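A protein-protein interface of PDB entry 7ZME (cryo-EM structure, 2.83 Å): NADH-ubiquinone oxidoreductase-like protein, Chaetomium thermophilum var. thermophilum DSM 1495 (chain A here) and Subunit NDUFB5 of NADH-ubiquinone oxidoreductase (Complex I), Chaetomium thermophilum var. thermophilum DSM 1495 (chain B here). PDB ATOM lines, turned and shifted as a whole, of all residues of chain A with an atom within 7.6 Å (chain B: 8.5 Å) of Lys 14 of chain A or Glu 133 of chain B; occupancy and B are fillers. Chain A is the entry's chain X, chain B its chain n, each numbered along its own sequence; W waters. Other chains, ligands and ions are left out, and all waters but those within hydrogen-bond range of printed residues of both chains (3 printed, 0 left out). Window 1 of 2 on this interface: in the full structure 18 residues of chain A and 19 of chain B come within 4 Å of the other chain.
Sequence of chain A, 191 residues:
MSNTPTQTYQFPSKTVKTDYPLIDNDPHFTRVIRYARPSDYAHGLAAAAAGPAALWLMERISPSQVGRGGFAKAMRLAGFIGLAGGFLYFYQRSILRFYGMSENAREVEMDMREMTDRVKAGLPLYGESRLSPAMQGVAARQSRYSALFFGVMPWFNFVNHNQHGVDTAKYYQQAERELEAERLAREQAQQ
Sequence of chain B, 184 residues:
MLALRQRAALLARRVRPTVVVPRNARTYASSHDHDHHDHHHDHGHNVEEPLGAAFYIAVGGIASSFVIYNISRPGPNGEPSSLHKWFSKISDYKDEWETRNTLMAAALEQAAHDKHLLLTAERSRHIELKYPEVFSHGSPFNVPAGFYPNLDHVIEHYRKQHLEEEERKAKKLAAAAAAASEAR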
ATOM      1  N   TYR A   9     -11.872  24.635  -4.559  1.00  0.00           N
ATOM      2  CA  TYR A   9     -12.423  24.664  -3.177  1.00  0.00           C
ATOM      3  C   TYR A   9     -12.800  26.123  -2.928  1.00  0.00           C
ATOM      4  O   TYR A   9     -11.883  26.922  -2.710  1.00  0.00           O
ATOM      5  CB  TYR A   9     -11.353  24.157  -2.214  1.00  0.00           C
ATOM      6  CG  TYR A   9     -11.780  23.699  -0.845  1.00  0.00           C
ATOM      7  CD1 TYR A   9     -12.092  22.373  -0.603  1.00  0.00           C
ATOM      8  CD2 TYR A   9     -11.790  24.573   0.225  1.00  0.00           C
ATOM      9  CE1 TYR A   9     -12.451  21.936   0.660  1.00  0.00           C
ATOM     10  CE2 TYR A   9     -12.145  24.155   1.494  1.00  0.00           C
ATOM     11  CZ  TYR A   9     -12.476  22.831   1.712  1.00  0.00           C
ATOM     12  OH  TYR A   9     -12.818  22.412   2.962  1.00  0.00           O
ATOM     13  N   PHE A  11     -15.569  27.202  -0.804  1.00  0.00           N
ATOM     14  CA  PHE A  11     -16.276  27.416   0.472  1.00  0.00           C
ATOM     15  C   PHE A  11     -15.484  26.710   1.554  1.00  0.00           C
ATOM     16  O   PHE A  11     -14.889  25.673   1.267  1.00  0.00           O
ATOM     17  CB  PHE A  11     -17.708  26.890   0.348  1.00  0.00           C
ATOM     18  CG  PHE A  11     -18.483  27.464  -0.808  1.00  0.00           C
ATOM     19  CD1 PHE A  11     -19.055  28.721  -0.719  1.00  0.00           C
ATOM     20  CD2 PHE A  11     -18.628  26.753  -1.987  1.00  0.00           C
ATOM     21  CE1 PHE A  11     -19.762  29.252  -1.785  1.00  0.00           C
ATOM     22  CE2 PHE A  11     -19.336  27.285  -3.052  1.00  0.00           C
ATOM     23  CZ  PHE A  11     -19.901  28.533  -2.948  1.00  0.00           C
ATOM     24  N   PRO A  12     -15.475  27.235   2.790  1.00  0.00           N
ATOM     25  CA  PRO A  12     -14.782  26.577   3.882  1.00  0.00           C
ATOM     26  C   PRO A  12     -15.625  25.420   4.437  1.00  0.00           C
ATOM     27  O   PRO A  12     -16.716  25.647   4.868  1.00  0.00           O
ATOM     28  CB  PRO A  12     -14.557  27.753   4.842  1.00  0.00           C
ATOM     29  CG  PRO A  12     -15.737  28.669   4.629  1.00  0.00           C
ATOM     30  CD  PRO A  12     -16.078  28.515   3.164  1.00  0.00           C
ATOM     31  N   SER A  13     -15.065  24.215   4.444  1.00  0.00           N
ATOM     32  CA  SER A  13     -15.835  23.014   4.864  1.00  0.00           C
ATOM     33  C   SER A  13     -15.297  22.467   6.175  1.00  0.00           C
ATOM     34  O   SER A  13     -14.219  22.890   6.579  1.00  0.00           O
ATOM     35  CB  SER A  13     -15.801  21.969   3.793  1.00  0.00           C
ATOM     36  OG  SER A  13     -16.095  22.544   2.531  1.00  0.00           O
ATOM     37  N   LYS A  14     -16.026  21.542   6.790  1.00  0.00           N
ATOM     38  CA  LYS A  14     -15.564  20.902   8.047  1.00  0.00           C
ATOM     39  C   LYS A  14     -14.909  19.573   7.700  1.00  0.00           C
ATOM     40  O   LYS A  14     -15.553  18.768   7.016  1.00  0.00           O
ATOM     41  CB  LYS A  14     -16.742  20.656   8.992  1.00  0.00           C
ATOM     42  CG  LYS A  14     -16.428  19.896  10.273  1.00  0.00           C
ATOM     43  CD  LYS A  14     -15.503  20.642  11.201  1.00  0.00           C
ATOM     44  CE  LYS A  14     -15.223  19.906  12.491  1.00  0.00           C
ATOM     45  NZ  LYS A  14     -14.341  20.700  13.378  1.00  0.00           N
ATOM     46  N   THR A  15     -13.711  19.346   8.240  1.00  0.00           N
ATOM     47  CA  THR A  15     -13.002  18.063   8.057  1.00  0.00           C
ATOM     48  C   THR A  15     -13.405  17.162   9.221  1.00  0.00           C
ATOM     49  O   THR A  15     -13.279  17.594  10.374  1.00  0.00           O
ATOM     50  CB  THR A  15     -11.487  18.294   8.015  1.00  0.00           C
ATOM     51  OG1 THR A  15     -11.198  18.999   6.808  1.00  0.00           O
ATOM     52  CG2 THR A  15     -10.680  17.017   8.078  1.00  0.00           C
ATOM     53  N   VAL A  16     -13.904  15.974   8.916  1.00  0.00           N
ATOM     54  CA  VAL A  16     -14.256  14.993   9.979  1.00  0.00           C
ATOM     55  C   VAL A  16     -13.256  13.843   9.860  1.00  0.00           C
ATOM     56  O   VAL A  16     -12.909  13.483   8.723  1.00  0.00           O
ATOM     57  CB  VAL A  16     -15.712  14.513   9.823  1.00  0.00           C
ATOM     58  CG1 VAL A  16     -16.139  13.619  10.973  1.00  0.00           C
ATOM     59  CG2 VAL A  16     -16.674  15.675   9.645  1.00  0.00           C
ATOM     60  N   LYS A  17     -12.774  13.321  10.990  1.00  0.00           N
ATOM     61  CA  LYS A  17     -11.882  12.138  10.920  1.00  0.00           C
ATOM     62  C   LYS A  17     -12.741  10.912  10.611  1.00  0.00           C
ATOM     63  O   LYS A  17     -13.593  10.574  11.438  1.00  0.00           O
ATOM     64  CB  LYS A  17     -11.111  11.979  12.228  1.00  0.00           C
ATOM     65  CG  LYS A  17     -10.215  10.751  12.325  1.00  0.00           C
ATOM     66  CD  LYS A  17      -8.869  10.935  11.663  1.00  0.00           C
ATOM     67  CE  LYS A  17      -7.899   9.819  11.987  1.00  0.00           C
ATOM     68  NZ  LYS A  17      -6.519  10.151  11.563  1.00  0.00           N
ATOM     69  N   LEU A  22     -13.866  10.865   1.454  1.00  0.00           N
ATOM     70  CA  LEU A  22     -15.137  11.625   1.448  1.00  0.00           C
ATOM     71  C   LEU A  22     -15.473  11.912  -0.018  1.00  0.00           C
ATOM     72  O   LEU A  22     -14.612  12.450  -0.722  1.00  0.00           O
ATOM     73  CB  LEU A  22     -14.965  12.915   2.256  1.00  0.00           C
ATOM     74  CG  LEU A  22     -15.976  14.029   1.967  1.00  0.00           C
ATOM     75  CD1 LEU A  22     -17.325  13.736   2.599  1.00  0.00           C
ATOM     76  CD2 LEU A  22     -15.459  15.378   2.437  1.00  0.00           C
ATOM     77  N   ASN A  25     -20.216  15.621   1.096  1.00  0.00           N
ATOM     78  CA  ASN A  25     -20.648  15.872   2.493  1.00  0.00           C
ATOM     79  C   ASN A  25     -22.140  16.174   2.433  1.00  0.00           C
ATOM     80  O   ASN A  25     -22.805  16.042   3.467  1.00  0.00           O
ATOM     81  CB  ASN A  25     -19.762  16.896   3.214  1.00  0.00           C
ATOM     82  CG  ASN A  25     -20.001  18.353   2.878  1.00  0.00           C
ATOM     83  OD1 ASN A  25     -20.790  18.695   2.002  1.00  0.00           O
ATOM     84  ND2 ASN A  25     -19.308  19.230   3.582  1.00  0.00           N
ATOM     85  N   GLY A 137     -26.347  28.108  -0.593  1.00  0.00           N
ATOM     86  CA  GLY A 137     -25.419  28.015   0.544  1.00  0.00           C
ATOM     87  C   GLY A 137     -26.137  27.709   1.828  1.00  0.00           C
ATOM     88  O   GLY A 137     -25.659  26.847   2.559  1.00  0.00           O
ATOM     89  N   ALA A 140     -26.897  23.974   1.544  1.00  0.00           N
ATOM     90  CA  ALA A 140     -25.684  23.170   1.804  1.00  0.00           C
ATOM     91  C   ALA A 140     -25.397  23.161   3.309  1.00  0.00           C
ATOM     92  O   ALA A 140     -25.171  22.082   3.852  1.00  0.00           O
ATOM     93  CB  ALA A 140     -24.552  23.797   1.043  1.00  0.00           C
ATOM     94  N   ARG A 141     -25.423  24.322   3.949  1.00  0.00           N
ATOM     95  CA  ARG A 141     -25.128  24.466   5.396  1.00  0.00           C
ATOM     96  C   ARG A 141     -26.141  23.677   6.227  1.00  0.00           C
ATOM     97  O   ARG A 141     -25.738  23.086   7.232  1.00  0.00           O
ATOM     98  CB  ARG A 141     -24.881  25.928   5.770  1.00  0.00           C
ATOM     99  CG  ARG A 141     -23.694  26.535   5.038  1.00  0.00           C
ATOM    100  CD  ARG A 141     -23.323  27.939   5.464  1.00  0.00           C
ATOM    101  NE  ARG A 141     -24.438  28.865   5.583  1.00  0.00           N
ATOM    102  CZ  ARG A 141     -24.744  29.803   4.697  1.00  0.00           C
ATOM    103  NH1 ARG A 141     -25.772  30.601   4.910  1.00  0.00           N
ATOM    104  NH2 ARG A 141     -24.017  29.948   3.605  1.00  0.00           N
ATOM    105  N   ARG A 144     -25.546  19.447   5.176  1.00  0.00           N
ATOM    106  CA  ARG A 144     -24.276  18.668   5.125  1.00  0.00           C
ATOM    107  C   ARG A 144     -24.121  17.836   6.405  1.00  0.00           C
ATOM    108  O   ARG A 144     -24.322  18.404   7.495  1.00  0.00           O
ATOM    109  CB  ARG A 144     -23.077  19.550   4.760  1.00  0.00           C
ATOM    110  CG  ARG A 144     -22.772  20.691   5.718  1.00  0.00           C
ATOM    111  CD  ARG A 144     -21.606  20.348   6.618  1.00  0.00           C
ATOM    112  NE  ARG A 144     -21.517  21.281   7.725  1.00  0.00           N
ATOM    113  CZ  ARG A 144     -20.718  21.118   8.765  1.00  0.00           C
ATOM    114  NH1 ARG A 144     -19.950  20.049   8.831  1.00  0.00           N
ATOM    115  NH2 ARG A 144     -20.688  22.013   9.732  1.00  0.00           N
ATOM    116  N   TYR A 145     -23.802  16.541   6.277  1.00  0.00           N
ATOM    117  CA  TYR A 145     -23.648  15.633   7.444  1.00  0.00           C
ATOM    118  C   TYR A 145     -24.964  15.509   8.215  1.00  0.00           C
ATOM    119  O   TYR A 145     -24.903  15.168   9.396  1.00  0.00           O
ATOM    120  CB  TYR A 145     -22.431  15.994   8.298  1.00  0.00           C
ATOM    121  CG  TYR A 145     -21.098  15.888   7.607  1.00  0.00           C
ATOM    122  CD1 TYR A 145     -20.683  14.707   7.016  1.00  0.00           C
ATOM    123  CD2 TYR A 145     -20.237  16.970   7.571  1.00  0.00           C
ATOM    124  CE1 TYR A 145     -19.453  14.610   6.391  1.00  0.00           C
ATOM    125  CE2 TYR A 145     -19.004  16.891   6.949  1.00  0.00           C
ATOM    126  CZ  TYR A 145     -18.611  15.706   6.358  1.00  0.00           C
ATOM    127  OH  TYR A 145     -17.395  15.632   5.748  1.00  0.00           O
ATOM    128  N   GLN A 163     -21.765  23.074  -3.215  1.00  0.00           N
ATOM    129  CA  GLN A 163     -20.921  23.143  -1.998  1.00  0.00           C
ATOM    130  C   GLN A 163     -20.887  21.759  -1.361  1.00  0.00           C
ATOM    131  O   GLN A 163     -21.755  21.496  -0.526  1.00  0.00           O
ATOM    132  CB  GLN A 163     -21.539  24.225  -1.124  1.00  0.00           C
ATOM    133  CG  GLN A 163     -20.721  24.634   0.071  1.00  0.00           C
ATOM    134  CD  GLN A 163     -21.421  25.777   0.754  1.00  0.00           C
ATOM    135  OE1 GLN A 163     -21.969  26.663   0.102  1.00  0.00           O
ATOM    136  NE2 GLN A 163     -21.420  25.757   2.076  1.00  0.00           N
ATOM    137  N   HIS A 164     -19.921  20.890  -1.767  1.00  0.00           N
ATOM    138  CA  HIS A 164     -19.989  19.487  -1.260  1.00  0.00           C
ATOM    139  C   HIS A 164     -18.770  19.080  -0.430  1.00  0.00           C
ATOM    140  O   HIS A 164     -18.634  17.873  -0.192  1.00  0.00           O
ATOM    141  CB  HIS A 164     -20.293  18.539  -2.416  1.00  0.00           C
ATOM    142  CG  HIS A 164     -21.567  18.884  -3.109  1.00  0.00           C
ATOM    143  ND1 HIS A 164     -22.761  18.275  -2.805  1.00  0.00           N
ATOM    144  CD2 HIS A 164     -21.850  19.806  -4.046  1.00  0.00           C
ATOM    145  CE1 HIS A 164     -23.717  18.778  -3.549  1.00  0.00           C
ATOM    146  NE2 HIS A 164     -23.185  19.719  -4.312  1.00  0.00           N
ATOM    147  N   GLY A 165     -17.891  20.020  -0.074  1.00  0.00           N
ATOM    148  CA  GLY A 165     -16.765  19.727   0.831  1.00  0.00           C
ATOM    149  C   GLY A 165     -15.568  19.084   0.167  1.00  0.00           C
ATOM    150  O   GLY A 165     -14.597  18.807   0.882  1.00  0.00           O
ATOM    151  N   ILE B 127      -9.484  26.031  20.050  1.00  0.00           N
ATOM    152  CA  ILE B 127     -10.859  25.693  19.606  1.00  0.00           C
ATOM    153  C   ILE B 127     -10.854  25.533  18.089  1.00  0.00           C
ATOM    154  O   ILE B 127     -10.374  26.438  17.410  1.00  0.00           O
ATOM    155  CB  ILE B 127     -11.845  26.799  20.034  1.00  0.00           C
ATOM    156  CG1 ILE B 127     -11.566  27.327  21.443  1.00  0.00           C
ATOM    157  CG2 ILE B 127     -13.287  26.345  19.867  1.00  0.00           C
ATOM    158  CD1 ILE B 127     -11.980  26.392  22.548  1.00  0.00           C
ATOM    159  N   GLU B 128     -11.408  24.297  17.645  1.00  0.00           N
ATOM    160  CA  GLU B 128     -11.611  24.074  16.187  1.00  0.00           C
ATOM    161  C   GLU B 128     -13.098  24.289  15.953  1.00  0.00           C
ATOM    162  O   GLU B 128     -13.867  23.626  16.639  1.00  0.00           O
ATOM    163  CB  GLU B 128     -11.177  22.659  15.805  1.00  0.00           C
ATOM    164  CG  GLU B 128     -11.296  22.338  14.335  1.00  0.00           C
ATOM    165  CD  GLU B 128     -10.054  22.678  13.537  1.00  0.00           C
ATOM    166  OE1 GLU B 128      -9.043  23.064  14.154  1.00  0.00           O
ATOM    167  OE2 GLU B 128     -10.105  22.559  12.299  1.00  0.00           O
ATOM    168  N   LEU B 129     -13.459  25.266  14.996  1.00  0.00           N
ATOM    169  CA  LEU B 129     -14.911  25.521  14.820  1.00  0.00           C
ATOM    170  C   LEU B 129     -15.621  24.229  14.418  1.00  0.00           C
ATOM    171  O   LEU B 129     -15.163  23.589  13.464  1.00  0.00           O
ATOM    172  CB  LEU B 129     -15.087  26.593  13.742  1.00  0.00           C
ATOM    173  CG  LEU B 129     -14.340  27.898  13.980  1.00  0.00           C
ATOM    174  CD1 LEU B 129     -14.543  28.849  12.816  1.00  0.00           C
ATOM    175  CD2 LEU B 129     -14.817  28.532  15.266  1.00  0.00           C
ATOM    176  N   LYS B 130     -16.677  23.848  15.135  1.00  0.00           N
ATOM    177  CA  LYS B 130     -17.506  22.675  14.768  1.00  0.00           C
ATOM    178  C   LYS B 130     -18.218  23.043  13.480  1.00  0.00           C
ATOM    179  O   LYS B 130     -18.507  22.141  12.683  1.00  0.00           O
ATOM    180  CB  LYS B 130     -18.580  22.425  15.828  1.00  0.00           C
ATOM    181  CG  LYS B 130     -18.096  21.927  17.180  1.00  0.00           C
ATOM    182  CD  LYS B 130     -19.194  21.903  18.218  1.00  0.00           C
ATOM    183  CE  LYS B 130     -18.749  21.302  19.534  1.00  0.00           C
ATOM    184  NZ  LYS B 130     -19.794  21.425  20.577  1.00  0.00           N
ATOM    185  N   TYR B 131     -18.492  24.341  13.312  1.00  0.00           N
ATOM    186  CA  TYR B 131     -19.189  24.865  12.111  1.00  0.00           C
ATOM    187  C   TYR B 131     -18.265  25.891  11.418  1.00  0.00           C
ATOM    188  O   TYR B 131     -18.465  27.084  11.630  1.00  0.00           O
ATOM    189  CB  TYR B 131     -20.580  25.338  12.521  1.00  0.00           C
ATOM    190  CG  TYR B 131     -21.455  25.890  11.429  1.00  0.00           C
ATOM    191  CD1 TYR B 131     -21.953  25.077  10.428  1.00  0.00           C
ATOM    192  CD2 TYR B 131     -21.826  27.222  11.433  1.00  0.00           C
ATOM    193  CE1 TYR B 131     -22.774  25.579   9.436  1.00  0.00           C
ATOM    194  CE2 TYR B 131     -22.650  27.739  10.453  1.00  0.00           C
ATOM    195  CZ  TYR B 131     -23.120  26.917   9.448  1.00  0.00           C
ATOM    196  OH  TYR B 131     -23.936  27.424   8.484  1.00  0.00           O
ATOM    197  N   PRO B 132     -17.242  25.485  10.617  1.00  0.00           N
ATOM    198  CA  PRO B 132     -16.390  26.432   9.890  1.00  0.00           C
ATOM    199  C   PRO B 132     -17.186  27.151   8.797  1.00  0.00           C
ATOM    200  O   PRO B 132     -16.666  28.081   8.249  1.00  0.00           O
ATOM    201  CB  PRO B 132     -15.399  25.508   9.165  1.00  0.00           C
ATOM    202  CG  PRO B 132     -15.415  24.234   9.953  1.00  0.00           C
ATOM    203  CD  PRO B 132     -16.854  24.097  10.386  1.00  0.00           C
ATOM    204  N   GLU B 133     -18.415  26.701   8.523  1.00  0.00           N
ATOM    205  CA  GLU B 133     -19.224  27.246   7.408  1.00  0.00           C
ATOM    206  C   GLU B 133     -19.867  28.547   7.871  1.00  0.00           C
ATOM    207  O   GLU B 133     -20.620  29.136   7.095  1.00  0.00           O
ATOM    208  CB  GLU B 133     -20.244  26.183   7.012  1.00  0.00           C
ATOM    209  CG  GLU B 133     -19.742  25.166   6.005  1.00  0.00           C
ATOM    210  CD  GLU B 133     -19.182  23.878   6.576  1.00  0.00           C
ATOM    211  OE1 GLU B 133     -18.885  23.851   7.778  1.00  0.00           O
ATOM    212  OE2 GLU B 133     -19.057  22.903   5.813  1.00  0.00           O
ATOM    213  N   VAL B 134     -19.596  28.953   9.107  1.00  0.00           N
ATOM    214  CA  VAL B 134     -20.024  30.268   9.560  1.00  0.00           C
ATOM    215  C   VAL B 134     -19.301  31.372   8.799  1.00  0.00           C
ATOM    216  O   VAL B 134     -19.772  32.513   8.770  1.00  0.00           O
ATOM    217  CB  VAL B 134     -19.801  30.388  11.081  1.00  0.00           C
ATOM    218  CG1 VAL B 134     -18.315  30.430  11.407  1.00  0.00           C
ATOM    219  CG2 VAL B 134     -20.533  31.586  11.652  1.00  0.00           C
ATOM    220  N   PHE B 135     -18.167  31.056   8.168  1.00  0.00           N
ATOM    221  CA  PHE B 135     -17.461  32.036   7.354  1.00  0.00           C
ATOM    222  C   PHE B 135     -18.236  32.406   6.100  1.00  0.00           C
ATOM    223  O   PHE B 135     -17.917  33.414   5.463  1.00  0.00           O
ATOM    224  CB  PHE B 135     -16.081  31.506   6.965  1.00  0.00           C
ATOM    225  CG  PHE B 135     -15.035  31.671   8.031  1.00  0.00           C
ATOM    226  CD1 PHE B 135     -14.596  32.930   8.400  1.00  0.00           C
ATOM    227  CD2 PHE B 135     -14.481  30.565   8.652  1.00  0.00           C
ATOM    228  CE1 PHE B 135     -13.629  33.082   9.375  1.00  0.00           C
ATOM    229  CE2 PHE B 135     -13.514  30.714   9.632  1.00  0.00           C
ATOM    230  CZ  PHE B 135     -13.087  31.971   9.990  1.00  0.00           C
ATOM    231  N   SER B 136     -19.239  31.615   5.733  1.00  0.00           N
ATOM    232  CA  SER B 136     -20.059  31.862   4.558  1.00  0.00           C
ATOM    233  C   SER B 136     -21.348  32.604   4.880  1.00  0.00           C
ATOM    234  O   SER B 136     -22.159  32.828   3.978  1.00  0.00           O
ATOM    235  CB  SER B 136     -20.384  30.541   3.863  1.00  0.00           C
ATOM    236  OG  SER B 136     -19.205  29.917   3.389  1.00  0.00           O
ATOM    237  N   HIS B 137     -21.533  32.969   6.146  1.00  0.00           N
ATOM    238  CA  HIS B 137     -22.752  33.688   6.586  1.00  0.00           C
ATOM    239  C   HIS B 137     -22.721  35.145   6.132  1.00  0.00           C
ATOM    240  O   HIS B 137     -21.702  35.575   5.562  1.00  0.00           O
ATOM    241  CB  HIS B 137     -22.875  33.609   8.110  1.00  0.00           C
ATOM    242  CG  HIS B 137     -23.382  32.303   8.611  1.00  0.00           C
ATOM    243  ND1 HIS B 137     -23.880  32.154   9.885  1.00  0.00           N
ATOM    244  CD2 HIS B 137     -23.479  31.097   8.020  1.00  0.00           C
ATOM    245  CE1 HIS B 137     -24.257  30.908  10.063  1.00  0.00           C
ATOM    246  NE2 HIS B 137     -24.025  30.245   8.932  1.00  0.00           N
ATOM    247  N   GLY B 138     -23.775  35.891   6.440  1.00  0.00           N
ATOM    248  CA  GLY B 138     -23.884  37.293   6.006  1.00  0.00           C
ATOM    249  C   GLY B 138     -24.955  37.474   4.955  1.00  0.00           C
ATOM    250  O   GLY B 138     -25.093  36.579   4.119  1.00  0.00           O
ATOM    251  N   TYR B 158      -8.633  25.868   5.206  1.00  0.00           N
ATOM    252  CA  TYR B 158      -9.595  24.742   5.160  1.00  0.00           C
ATOM    253  C   TYR B 158      -9.321  23.848   3.951  1.00  0.00           C
ATOM    254  O   TYR B 158      -9.478  22.630   4.077  1.00  0.00           O
ATOM    255  CB  TYR B 158     -11.021  25.273   5.306  1.00  0.00           C
ATOM    256  CG  TYR B 158     -11.348  25.767   6.689  1.00  0.00           C
ATOM    257  CD1 TYR B 158     -11.385  24.897   7.764  1.00  0.00           C
ATOM    258  CD2 TYR B 158     -11.622  27.103   6.928  1.00  0.00           C
ATOM    259  CE1 TYR B 158     -11.681  25.339   9.041  1.00  0.00           C
ATOM    260  CE2 TYR B 158     -11.926  27.562   8.198  1.00  0.00           C
ATOM    261  CZ  TYR B 158     -11.957  26.676   9.257  1.00  0.00           C
ATOM    262  OH  TYR B 158     -12.261  27.117  10.509  1.00  0.00           O
ATOM    263  N   GLN B 161      -6.518  21.533   5.185  1.00  0.00           N
ATOM    264  CA  GLN B 161      -7.024  20.509   6.137  1.00  0.00           C
ATOM    265  C   GLN B 161      -7.698  19.385   5.351  1.00  0.00           C
ATOM    266  O   GLN B 161      -7.419  18.221   5.661  1.00  0.00           O
ATOM    267  CB  GLN B 161      -7.998  21.153   7.119  1.00  0.00           C
ATOM    268  CG  GLN B 161      -8.276  20.330   8.363  1.00  0.00           C
ATOM    269  CD  GLN B 161      -9.150  21.090   9.330  1.00  0.00           C
ATOM    270  OE1 GLN B 161      -9.720  20.524  10.259  1.00  0.00           O
ATOM    271  NE2 GLN B 161      -9.262  22.390   9.114  1.00  0.00           N
ATOM    272  N   HIS B 162      -8.582  19.718   4.409  1.00  0.00           N
ATOM    273  CA  HIS B 162      -9.238  18.684   3.572  1.00  0.00           C
ATOM    274  C   HIS B 162      -8.206  17.898   2.762  1.00  0.00           C
ATOM    275  O   HIS B 162      -8.255  16.670   2.808  1.00  0.00           O
ATOM    276  CB  HIS B 162     -10.280  19.333   2.655  1.00  0.00           C
ATOM    277  CG  HIS B 162     -10.873  18.410   1.648  1.00  0.00           C
ATOM    278  ND1 HIS B 162     -11.677  17.351   2.004  1.00  0.00           N
ATOM    279  CD2 HIS B 162     -10.792  18.392   0.303  1.00  0.00           C
ATOM    280  CE1 HIS B 162     -12.062  16.714   0.919  1.00  0.00           C
ATOM    281  NE2 HIS B 162     -11.529  17.331  -0.135  1.00  0.00           N
ATOM    282  N   GLU B 165      -6.239  15.609   5.091  1.00  0.00           N
ATOM    283  CA  GLU B 165      -7.000  14.469   5.660  1.00  0.00           C
ATOM    284  C   GLU B 165      -7.118  13.390   4.588  1.00  0.00           C
ATOM    285  O   GLU B 165      -6.833  12.236   4.891  1.00  0.00           O
ATOM    286  CB  GLU B 165      -8.374  14.950   6.130  1.00  0.00           C
ATOM    287  CG  GLU B 165      -9.408  13.850   6.296  1.00  0.00           C
ATOM    288  CD  GLU B 165      -9.440  13.168   7.652  1.00  0.00           C
ATOM    289  OE1 GLU B 165      -8.784  13.672   8.585  1.00  0.00           O
ATOM    290  OE2 GLU B 165     -10.119  12.130   7.771  1.00  0.00           O
ATOM    291  N   GLU B 166      -7.565  13.763   3.391  1.00  0.00           N
ATOM    292  CA  GLU B 166      -7.746  12.809   2.272  1.00  0.00           C
ATOM    293  C   GLU B 166      -6.402  12.197   1.868  1.00  0.00           C
ATOM    294  O   GLU B 166      -6.374  11.013   1.555  1.00  0.00           O
ATOM    295  CB  GLU B 166      -8.388  13.547   1.098  1.00  0.00           C
ATOM    296  CG  GLU B 166      -9.706  14.220   1.444  1.00  0.00           C
ATOM    297  CD  GLU B 166     -10.756  13.394   2.171  1.00  0.00           C
ATOM    298  OE1 GLU B 166     -10.986  12.234   1.775  1.00  0.00           O
ATOM    299  OE2 GLU B 166     -11.344  13.919   3.139  1.00  0.00           O
HETATM  300  O   HOH W   1     -11.479  21.781   6.248  1.00  0.00           O
HETATM  301  O   HOH W   2     -19.093  27.243   3.645  1.00  0.00           O
HETATM  302  O   HOH W   3     -12.578  21.805   9.478  1.00  0.00           O
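Water W2 lies within hydrogen-bond range of OG of Ser 136 of chain B (2.7 Å), O of Pro 12 of chain A (3.1 Å) and NE2 of Gln 163 of chain A (3.2 Å).
The side-chain carboxylate (OE2) of Glu 165 of chain B lies close to the backbone carbonyl oxygen (O) of Val 16 of chain A (3.2 Å).
The backbone carbonyl oxygen of Gly 165 of chain A lies close to a ring nitrogen (ND1) of His 162 of chain B, 3.5 Å away.
The side-chain carboxylate of Glu 133 of chain B is in hydrogen-bond range of the backbone NH of Lys 14 of chain A, 3.5 Å away.
NH2 of Arg 141 of chain A is in hydrogen-bond range of O of Ser 136 of chain B, at 3.4 Å.
The side-chain amino group (NZ) of Lys 14 of chain A is in hydrogen-bond range of the backbone carbonyl oxygen (O) of Leu 129 of chain B, 3.0 Å away.
The guanidinium group (NH2) of Arg 144 of chain A is in salt-bridge range of the side-chain carboxylate (OE1) of Glu 133 of chain B.
The guanidinium group (NE) of Arg 141 of chain A sits close to the side-chain hydroxyl (OH) of Tyr 131 of chain B (3.3 Å).
The backbone NH (N) of Leu 22 of chain A sits at hydrogen-bond distance from the side-chain carboxylate (OE1) of Glu 166 of chain B, 3.2 Å away.
Hydrophobic or aromatic side chains of chain A that line the printed part of chain B: Tyr 9, Pro 12 and Leu 22.
Of the 17 printed residues of chain B, 14 touch a printed residue of chain A.
Among the printed residues, 30 pairs touch across the chains.
Lys 14 of chain A touches five residues of chain B.
Of chain A, only Pro 12, Ser 13, Lys 14, Arg 141 and Arg 144 come within 4 Å of Glu 133 of chain B.
Of the printed residues of chain A, Glu 128 of chain B touches Lys 14 (3.6 Å).
Ile 127 of chain B touches none of the printed residues of chain A.
Gly 138 of chain B touches none of the printed residues of chain A.
The nearest residue of chain B that does not touch Lys 14 of chain A is Tyr 131 of chain B (5.2 Å).
A ring nitrogen (NE2) of His 137 of chain B is in hydrogen-bond range of the side-chain hydroxyl of Tyr 131 of chain B (2.9 Å).
The side-chain carboxylate of Glu 128 of chain B sits close to the side-chain amide oxygen of Gln 161 of chain B.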
